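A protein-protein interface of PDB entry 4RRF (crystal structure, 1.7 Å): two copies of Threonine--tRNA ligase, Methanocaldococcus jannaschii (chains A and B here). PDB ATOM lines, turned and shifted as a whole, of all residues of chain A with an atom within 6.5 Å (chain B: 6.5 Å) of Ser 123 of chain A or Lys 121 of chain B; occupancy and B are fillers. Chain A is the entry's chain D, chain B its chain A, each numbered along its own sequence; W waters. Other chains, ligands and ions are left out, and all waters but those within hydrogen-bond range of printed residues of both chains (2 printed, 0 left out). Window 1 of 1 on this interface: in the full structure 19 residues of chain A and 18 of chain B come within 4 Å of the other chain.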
ATOM      1  N   ILE A   6      21.797   7.941 -25.191  1.00  0.00           N
ATOM      2  CA  ILE A   6      21.351   9.017 -26.078  1.00  0.00           C
ATOM      3  C   ILE A   6      22.514   9.635 -26.846  1.00  0.00           C
ATOM      4  O   ILE A   6      23.464  10.148 -26.245  1.00  0.00           O
ATOM      5  CB  ILE A   6      20.616  10.144 -25.293  1.00  0.00           C
ATOM      6  CG1 ILE A   6      19.450   9.545 -24.460  1.00  0.00           C
ATOM      7  CG2 ILE A   6      20.182  11.305 -26.221  1.00  0.00           C
ATOM      8  CD1 ILE A   6      18.342  10.504 -24.033  1.00  0.00           C
ATOM      9  N   HIS A   7      22.442   9.591 -28.168  1.00  0.00           N
ATOM     10  CA  HIS A   7      23.498  10.161 -29.033  1.00  0.00           C
ATOM     11  C   HIS A   7      23.318  11.638 -29.160  1.00  0.00           C
ATOM     12  O   HIS A   7      22.267  12.077 -29.673  1.00  0.00           O
ATOM     13  CB  HIS A   7      23.454   9.508 -30.422  1.00  0.00           C
ATOM     14  CG  HIS A   7      24.595   9.915 -31.302  1.00  0.00           C
ATOM     15  ND1 HIS A   7      24.528   9.857 -32.656  1.00  0.00           N
ATOM     16  CD2 HIS A   7      25.832  10.435 -30.991  1.00  0.00           C
ATOM     17  CE1 HIS A   7      25.694  10.284 -33.180  1.00  0.00           C
ATOM     18  NE2 HIS A   7      26.492  10.668 -32.155  1.00  0.00           N
ATOM     19  N   SER A   8      24.277  12.366 -28.611  1.00  0.00           N
ATOM     20  CA  SER A   8      24.082  13.825 -28.372  1.00  0.00           C
ATOM     21  C   SER A   8      25.099  14.757 -29.042  1.00  0.00           C
ATOM     22  O   SER A   8      26.269  14.477 -29.083  1.00  0.00           O
ATOM     23  CB  SER A   8      24.089  14.141 -26.880  1.00  0.00           C
ATOM     24  OG  SER A   8      23.091  13.402 -26.186  1.00  0.00           O
ATOM     25  N   ASP A   9      24.648  15.906 -29.520  1.00  0.00           N
ATOM     26  CA  ASP A   9      25.574  17.001 -29.900  1.00  0.00           C
ATOM     27  C   ASP A   9      26.350  17.453 -28.697  1.00  0.00           C
ATOM     28  O   ASP A   9      27.553  17.737 -28.791  1.00  0.00           O
ATOM     29  CB  ASP A   9      24.794  18.196 -30.475  1.00  0.00           C
ATOM     30  CG  ASP A   9      23.882  17.793 -31.605  1.00  0.00           C
ATOM     31  OD1 ASP A   9      24.394  17.565 -32.742  1.00  0.00           O
ATOM     32  OD2 ASP A   9      22.652  17.754 -31.363  1.00  0.00           O
ATOM     33  N   TYR A  10      25.691  17.450 -27.535  1.00  0.00           N
ATOM     34  CA  TYR A  10      26.358  17.736 -26.266  1.00  0.00           C
ATOM     35  C   TYR A  10      25.513  17.305 -25.076  1.00  0.00           C
ATOM     36  O   TYR A  10      24.280  17.212 -25.168  1.00  0.00           O
ATOM     37  CB  TYR A  10      26.626  19.230 -26.124  1.00  0.00           C
ATOM     38  CG  TYR A  10      25.393  20.105 -26.237  1.00  0.00           C
ATOM     39  CD1 TYR A  10      24.501  20.235 -25.145  1.00  0.00           C
ATOM     40  CD2 TYR A  10      25.050  20.711 -27.452  1.00  0.00           C
ATOM     41  CE1 TYR A  10      23.339  21.004 -25.272  1.00  0.00           C
ATOM     42  CE2 TYR A  10      23.926  21.490 -27.572  1.00  0.00           C
ATOM     43  CZ  TYR A  10      23.091  21.651 -26.477  1.00  0.00           C
ATOM     44  OH  TYR A  10      21.944  22.415 -26.599  1.00  0.00           O
ATOM     45  N   LEU A  11      26.184  17.165 -23.936  1.00  0.00           N
ATOM     46  CA  LEU A  11      25.524  16.946 -22.647  1.00  0.00           C
ATOM     47  C   LEU A  11      26.259  17.944 -21.710  1.00  0.00           C
ATOM     48  O   LEU A  11      27.521  17.998 -21.742  1.00  0.00           O
ATOM     49  CB  LEU A  11      25.680  15.530 -22.147  1.00  0.00           C
ATOM     50  CG  LEU A  11      25.035  15.267 -20.771  1.00  0.00           C
ATOM     51  CD1 LEU A  11      24.597  13.833 -20.646  1.00  0.00           C
ATOM     52  CD2 LEU A  11      25.915  15.691 -19.577  1.00  0.00           C
ATOM     53  N   LYS A 121      21.694  20.047 -19.652  1.00  0.00           N
ATOM     54  CA  LYS A 121      21.246  20.413 -20.980  1.00  0.00           C
ATOM     55  C   LYS A 121      21.697  19.300 -21.890  1.00  0.00           C
ATOM     56  O   LYS A 121      22.779  18.791 -21.708  1.00  0.00           O
ATOM     57  CB  LYS A 121      21.867  21.730 -21.432  1.00  0.00           C
ATOM     58  CG  LYS A 121      21.569  22.914 -20.522  1.00  0.00           C
ATOM     59  CD  LYS A 121      22.096  24.172 -21.231  1.00  0.00           C
ATOM     60  CE  LYS A 121      21.938  25.409 -20.361  1.00  0.00           C
ATOM     61  NZ  LYS A 121      22.720  26.490 -21.009  1.00  0.00           N
ATOM     62  N   ILE A 122      20.836  18.893 -22.818  1.00  0.00           N
ATOM     63  CA  ILE A 122      21.192  17.799 -23.754  1.00  0.00           C
ATOM     64  C   ILE A 122      20.614  18.154 -25.127  1.00  0.00           C
ATOM     65  O   ILE A 122      19.530  18.795 -25.234  1.00  0.00           O
ATOM     66  CB  ILE A 122      20.751  16.409 -23.265  1.00  0.00           C
ATOM     67  CG1 ILE A 122      21.271  15.293 -24.178  1.00  0.00           C
ATOM     68  CG2 ILE A 122      19.240  16.290 -23.288  1.00  0.00           C
ATOM     69  CD1 ILE A 122      21.326  13.916 -23.472  1.00  0.00           C
ATOM     70  N   SER A 123      21.326  17.813 -26.193  1.00  0.00           N
ATOM     71  CA  SER A 123      20.750  17.948 -27.540  1.00  0.00           C
ATOM     72  C   SER A 123      20.894  16.587 -28.189  1.00  0.00           C
ATOM     73  O   SER A 123      22.052  16.159 -28.463  1.00  0.00           O
ATOM     74  CB  SER A 123      21.475  19.046 -28.362  1.00  0.00           C
ATOM     75  OG  SER A 123      21.167  18.982 -29.743  1.00  0.00           O
ATOM     76  N   CYS A 124      19.756  15.913 -28.395  1.00  0.00           N
ATOM     77  CA  CYS A 124      19.723  14.527 -28.965  1.00  0.00           C
ATOM     78  C   CYS A 124      19.622  14.601 -30.490  1.00  0.00           C
ATOM     79  O   CYS A 124      18.811  15.319 -31.010  1.00  0.00           O
ATOM     80  CB  CYS A 124      18.530  13.737 -28.401  1.00  0.00           C
ATOM     81  SG  CYS A 124      18.106  12.279 -29.402  1.00  0.00           S
ATOM     82  N   LYS A 125      20.501  13.904 -31.215  1.00  0.00           N
ATOM     83  CA  LYS A 125      20.560  14.062 -32.676  1.00  0.00           C
ATOM     84  C   LYS A 125      19.291  13.595 -33.473  1.00  0.00           C
ATOM     85  O   LYS A 125      19.055  14.084 -34.575  1.00  0.00           O
ATOM     86  CB  LYS A 125      21.826  13.400 -33.245  1.00  0.00           C
ATOM     87  CG  LYS A 125      23.116  13.956 -32.649  1.00  0.00           C
ATOM     88  CD  LYS A 125      24.317  13.574 -33.517  1.00  0.00           C
ATOM     89  CE  LYS A 125      25.606  14.035 -32.865  1.00  0.00           C
ATOM     90  NZ  LYS A 125      25.759  15.467 -33.206  1.00  0.00           N
ATOM     91  N   TYR B  10      13.455  25.219 -21.412  1.00  0.00           N
ATOM     92  CA  TYR B  10      12.872  25.105 -22.756  1.00  0.00           C
ATOM     93  C   TYR B  10      12.910  23.664 -23.183  1.00  0.00           C
ATOM     94  O   TYR B  10      13.748  22.865 -22.686  1.00  0.00           O
ATOM     95  CB  TYR B  10      13.685  25.985 -23.785  1.00  0.00           C
ATOM     96  CG  TYR B  10      15.171  25.603 -23.887  1.00  0.00           C
ATOM     97  CD1 TYR B  10      15.598  24.430 -24.559  1.00  0.00           C
ATOM     98  CD2 TYR B  10      16.170  26.408 -23.291  1.00  0.00           C
ATOM     99  CE1 TYR B  10      16.956  24.086 -24.591  1.00  0.00           C
ATOM    100  CE2 TYR B  10      17.519  26.066 -23.322  1.00  0.00           C
ATOM    101  CZ  TYR B  10      17.910  24.926 -23.985  1.00  0.00           C
ATOM    102  OH  TYR B  10      19.284  24.596 -23.966  1.00  0.00           O
ATOM    103  N   LEU B  11      12.017  23.295 -24.088  1.00  0.00           N
ATOM    104  CA  LEU B  11      12.110  22.026 -24.791  1.00  0.00           C
ATOM    105  C   LEU B  11      11.886  22.341 -26.284  1.00  0.00           C
ATOM    106  O   LEU B  11      10.891  23.025 -26.640  1.00  0.00           O
ATOM    107  CB  LEU B  11      11.040  21.054 -24.262  1.00  0.00           C
ATOM    108  CG  LEU B  11      10.925  19.658 -24.885  1.00  0.00           C
ATOM    109  CD1 LEU B  11      12.256  18.911 -24.852  1.00  0.00           C
ATOM    110  CD2 LEU B  11       9.908  18.856 -24.096  1.00  0.00           C
ATOM    111  N   GLU B  12      12.817  21.945 -27.145  1.00  0.00           N
ATOM    112  CA  GLU B  12      12.660  22.169 -28.584  1.00  0.00           C
ATOM    113  C   GLU B  12      12.762  20.847 -29.262  1.00  0.00           C
ATOM    114  O   GLU B  12      13.564  20.035 -28.822  1.00  0.00           O
ATOM    115  CB  GLU B  12      13.816  23.029 -29.123  1.00  0.00           C
ATOM    116  CG  GLU B  12      13.819  24.449 -28.616  1.00  0.00           C
ATOM    117  CD  GLU B  12      14.809  25.297 -29.389  1.00  0.00           C
ATOM    118  OE1 GLU B  12      15.728  24.702 -29.981  1.00  0.00           O
ATOM    119  OE2 GLU B  12      14.671  26.533 -29.374  1.00  0.00           O
ATOM    120  N   PHE B  13      11.968  20.598 -30.290  1.00  0.00           N
ATOM    121  CA  PHE B  13      12.110  19.310 -30.963  1.00  0.00           C
ATOM    122  C   PHE B  13      11.892  19.460 -32.482  1.00  0.00           C
ATOM    123  O   PHE B  13      11.232  20.402 -32.962  1.00  0.00           O
ATOM    124  CB  PHE B  13      11.142  18.237 -30.381  1.00  0.00           C
ATOM    125  CG  PHE B  13       9.701  18.565 -30.591  1.00  0.00           C
ATOM    126  CD1 PHE B  13       9.080  18.309 -31.834  1.00  0.00           C
ATOM    127  CD2 PHE B  13       8.953  19.113 -29.554  1.00  0.00           C
ATOM    128  CE1 PHE B  13       7.760  18.689 -32.040  1.00  0.00           C
ATOM    129  CE2 PHE B  13       7.606  19.424 -29.741  1.00  0.00           C
ATOM    130  CZ  PHE B  13       7.029  19.185 -30.998  1.00  0.00           C
ATOM    131  N   ALA B 119      14.720  14.810 -33.017  1.00  0.00           N
ATOM    132  CA  ALA B 119      15.811  15.524 -32.385  1.00  0.00           C
ATOM    133  C   ALA B 119      15.169  16.377 -31.325  1.00  0.00           C
ATOM    134  O   ALA B 119      14.042  16.786 -31.499  1.00  0.00           O
ATOM    135  CB  ALA B 119      16.591  16.371 -33.371  1.00  0.00           C
ATOM    136  N   PHE B 120      15.847  16.588 -30.201  1.00  0.00           N
ATOM    137  CA  PHE B 120      15.311  17.514 -29.230  1.00  0.00           C
ATOM    138  C   PHE B 120      16.427  18.144 -28.454  1.00  0.00           C
ATOM    139  O   PHE B 120      17.517  17.595 -28.352  1.00  0.00           O
ATOM    140  CB  PHE B 120      14.294  16.814 -28.277  1.00  0.00           C
ATOM    141  CG  PHE B 120      14.905  15.950 -27.201  1.00  0.00           C
ATOM    142  CD1 PHE B 120      15.173  14.603 -27.439  1.00  0.00           C
ATOM    143  CD2 PHE B 120      15.220  16.467 -25.926  1.00  0.00           C
ATOM    144  CE1 PHE B 120      15.744  13.789 -26.446  1.00  0.00           C
ATOM    145  CE2 PHE B 120      15.769  15.640 -24.932  1.00  0.00           C
ATOM    146  CZ  PHE B 120      16.040  14.312 -25.198  1.00  0.00           C
ATOM    147  N   LYS B 121      16.110  19.273 -27.844  1.00  0.00           N
ATOM    148  CA  LYS B 121      17.028  19.964 -26.976  1.00  0.00           C
ATOM    149  C   LYS B 121      16.214  20.338 -25.767  1.00  0.00           C
ATOM    150  O   LYS B 121      15.053  20.819 -25.865  1.00  0.00           O
ATOM    151  CB  LYS B 121      17.556  21.224 -27.633  1.00  0.00           C
ATOM    152  CG  LYS B 121      18.224  20.962 -28.967  1.00  0.00           C
ATOM    153  CD  LYS B 121      18.689  22.250 -29.648  1.00  0.00           C
ATOM    154  CE  LYS B 121      19.114  21.904 -31.076  1.00  0.00           C
ATOM    155  NZ  LYS B 121      19.758  23.028 -31.803  1.00  0.00           N
ATOM    156  N   ILE B 122      16.840  20.162 -24.613  1.00  0.00           N
ATOM    157  CA  ILE B 122      16.157  20.414 -23.328  1.00  0.00           C
ATOM    158  C   ILE B 122      17.182  21.059 -22.371  1.00  0.00           C
ATOM    159  O   ILE B 122      18.377  20.767 -22.433  1.00  0.00           O
ATOM    160  CB  ILE B 122      15.528  19.143 -22.736  1.00  0.00           C
ATOM    161  CG1 ILE B 122      14.600  19.470 -21.549  1.00  0.00           C
ATOM    162  CG2 ILE B 122      16.576  18.181 -22.196  1.00  0.00           C
ATOM    163  CD1 ILE B 122      13.584  18.361 -21.192  1.00  0.00           C
ATOM    164  N   SER B 123      16.683  21.899 -21.468  1.00  0.00           N
ATOM    165  CA  SER B 123      17.484  22.377 -20.382  1.00  0.00           C
ATOM    166  C   SER B 123      16.683  22.246 -19.094  1.00  0.00           C
ATOM    167  O   SER B 123      15.642  22.920 -18.939  1.00  0.00           O
ATOM    168  CB  SER B 123      17.787  23.843 -20.618  1.00  0.00           C
ATOM    169  OG  SER B 123      18.455  24.420 -19.503  1.00  0.00           O
HETATM  170  O   HOH W   1      18.790  18.383 -31.280  1.00  0.00           O
HETATM  171  O   HOH W   2      19.937  22.320 -24.977  1.00  0.00           O
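The backbone NH (N) of Ser 123 of chain B lies within hydrogen-bond range of the backbone carbonyl oxygen (O) of Tyr 10 of chain B, 3.3 Å away. The backbone carbonyl oxygen of Lys 121 of chain B sits at hydrogen-bond distance from the backbone NH of Glu 12 of chain B, at 2.8 Å. The backbone NH (N) of Lys 125 of chain A lies within hydrogen-bond range of the backbone carbonyl oxygen (O) of His 7 of chain A (3.0 Å). The side-chain hydroxyl of Ser 123 of chain A sits at hydrogen-bond distance from the side-chain carboxylate of Asp 9 of chain A, at 2.5 Å. The side-chain carboxylate (OD1) of Asp 9 of chain A is in salt-bridge range of the side-chain amino group (NZ) of Lys 125 of chain A. The backbone NH of Ser 123 of chain A sits at hydrogen-bond distance from the backbone carbonyl oxygen of Tyr 10 of chain A (3.2 Å).
Among the printed residues, merely in contact across the chains: Lys 121 of chain A with Tyr 10 of chain B, Lys 121 of chain A with Ile 122 of chain B, Lys 121 of chain A with Ser 123 of chain B, Ile 122 of chain A with Phe 120 of chain B, Ile 122 of chain A with Lys 121 of chain B, Ser 123 of chain A with Phe 120 of chain B, Ser 123 of chain A with Lys 121 of chain B, Cys 124 of chain A with Ala 119 of chain B and Lys 125 of chain A with Ala 119 of chain B.
Water W2 lies within hydrogen-bond range of OH of Tyr 10 of chain B, OH of Tyr 10 of chain A and O of Ile 122 of chain B. Water W1 lies within hydrogen-bond range of the side-chain hydroxyl (OG) of Ser 123 of chain A (2.9 Å), the backbone carbonyl oxygen (O) of Cys 124 of chain A (3.1 Å) and the backbone carbonyl oxygen (O) of Phe 120 of chain B (3.3 Å).
Lys 121 of chain A touches Tyr 10 of chain B, but with the chains exchanged Tyr 10 of chain A does not touch Lys 121 of chain B (4.5 Å). Lys 121 of chain A touches Ile 122 of chain B, and with the chains exchanged Ile 122 of chain A touches Lys 121 of chain B. Lys 121 of chain A touches Ser 123 of chain B, and with the chains exchanged Ser 123 of chain A touches Lys 121 of chain B. Ile 122 of chain A touches its own counterpart, Ile 122 of chain B. Of the 11 pairs that touch across the chains among the printed residues, 5 have their exchanged pair printed and touching as well.
Of the 9 printed residues of chain B, 6 touch a printed residue of chain A. Printed residues of chain B that touch a printed residue of chain A: Tyr 10, Ala 119, Phe 120, Lys 121, Ile 122 and Ser 123. Hydrophobic or aromatic side chains of chain A that line the printed part of chain B: Ile 122.
The backbone carbonyl oxygen (O) of Phe 120 of chain B lies within hydrogen-bond range of the backbone NH (N) of Cys 124 of chain A (2.8 Å). The backbone NH (N) of Ile 122 of chain B is in hydrogen-bond range of the backbone carbonyl oxygen (O) of Ile 122 of chain A (3.1 Å).
Ser 123 of chain A touches just these residues of chain B: Phe 120 (3.4 Å) and Lys 121 (3.6 Å). Lys 121 of chain B touches two residues of chain A. Of the printed residues of chain A, Ala 119 of chain B touches Cys 124 (3.3 Å) and Lys 125 (3.6 Å). Printed residues of chain B within 4 Å of Lys 121 of chain A: Tyr 10, Ile 122 and Ser 123. Of the printed residues of chain A, Phe 120 of chain B touches Ile 122 (3.9 Å), Ser 123 (3.4 Å) and Cys 124 (2.8 Å). Printed residues of chain B within 4 Å of Lys 125 of chain A: Ala 119 (3.6 Å). Of the printed residues of chain B, Ile 122 of chain A touches Phe 120 (3.9 Å), Lys 121 (3.3 Å) and Ile 122 (3.1 Å). Glu 12 of chain B touches none of the printed residues of chain A. Leu 11 of chain B touches none of the printed residues of chain A. The nearest residue of chain B that does not touch Ser 123 of chain A is Ile 122 of chain B (5.3 Å). The nearest residue of chain A that does not touch Lys 121 of chain B is Tyr 10 of chain A (4.5 Å). The nearest printed residue of chain B that does not touch Lys 121 of chain A is Lys 121 of chain B (6.8 Å).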
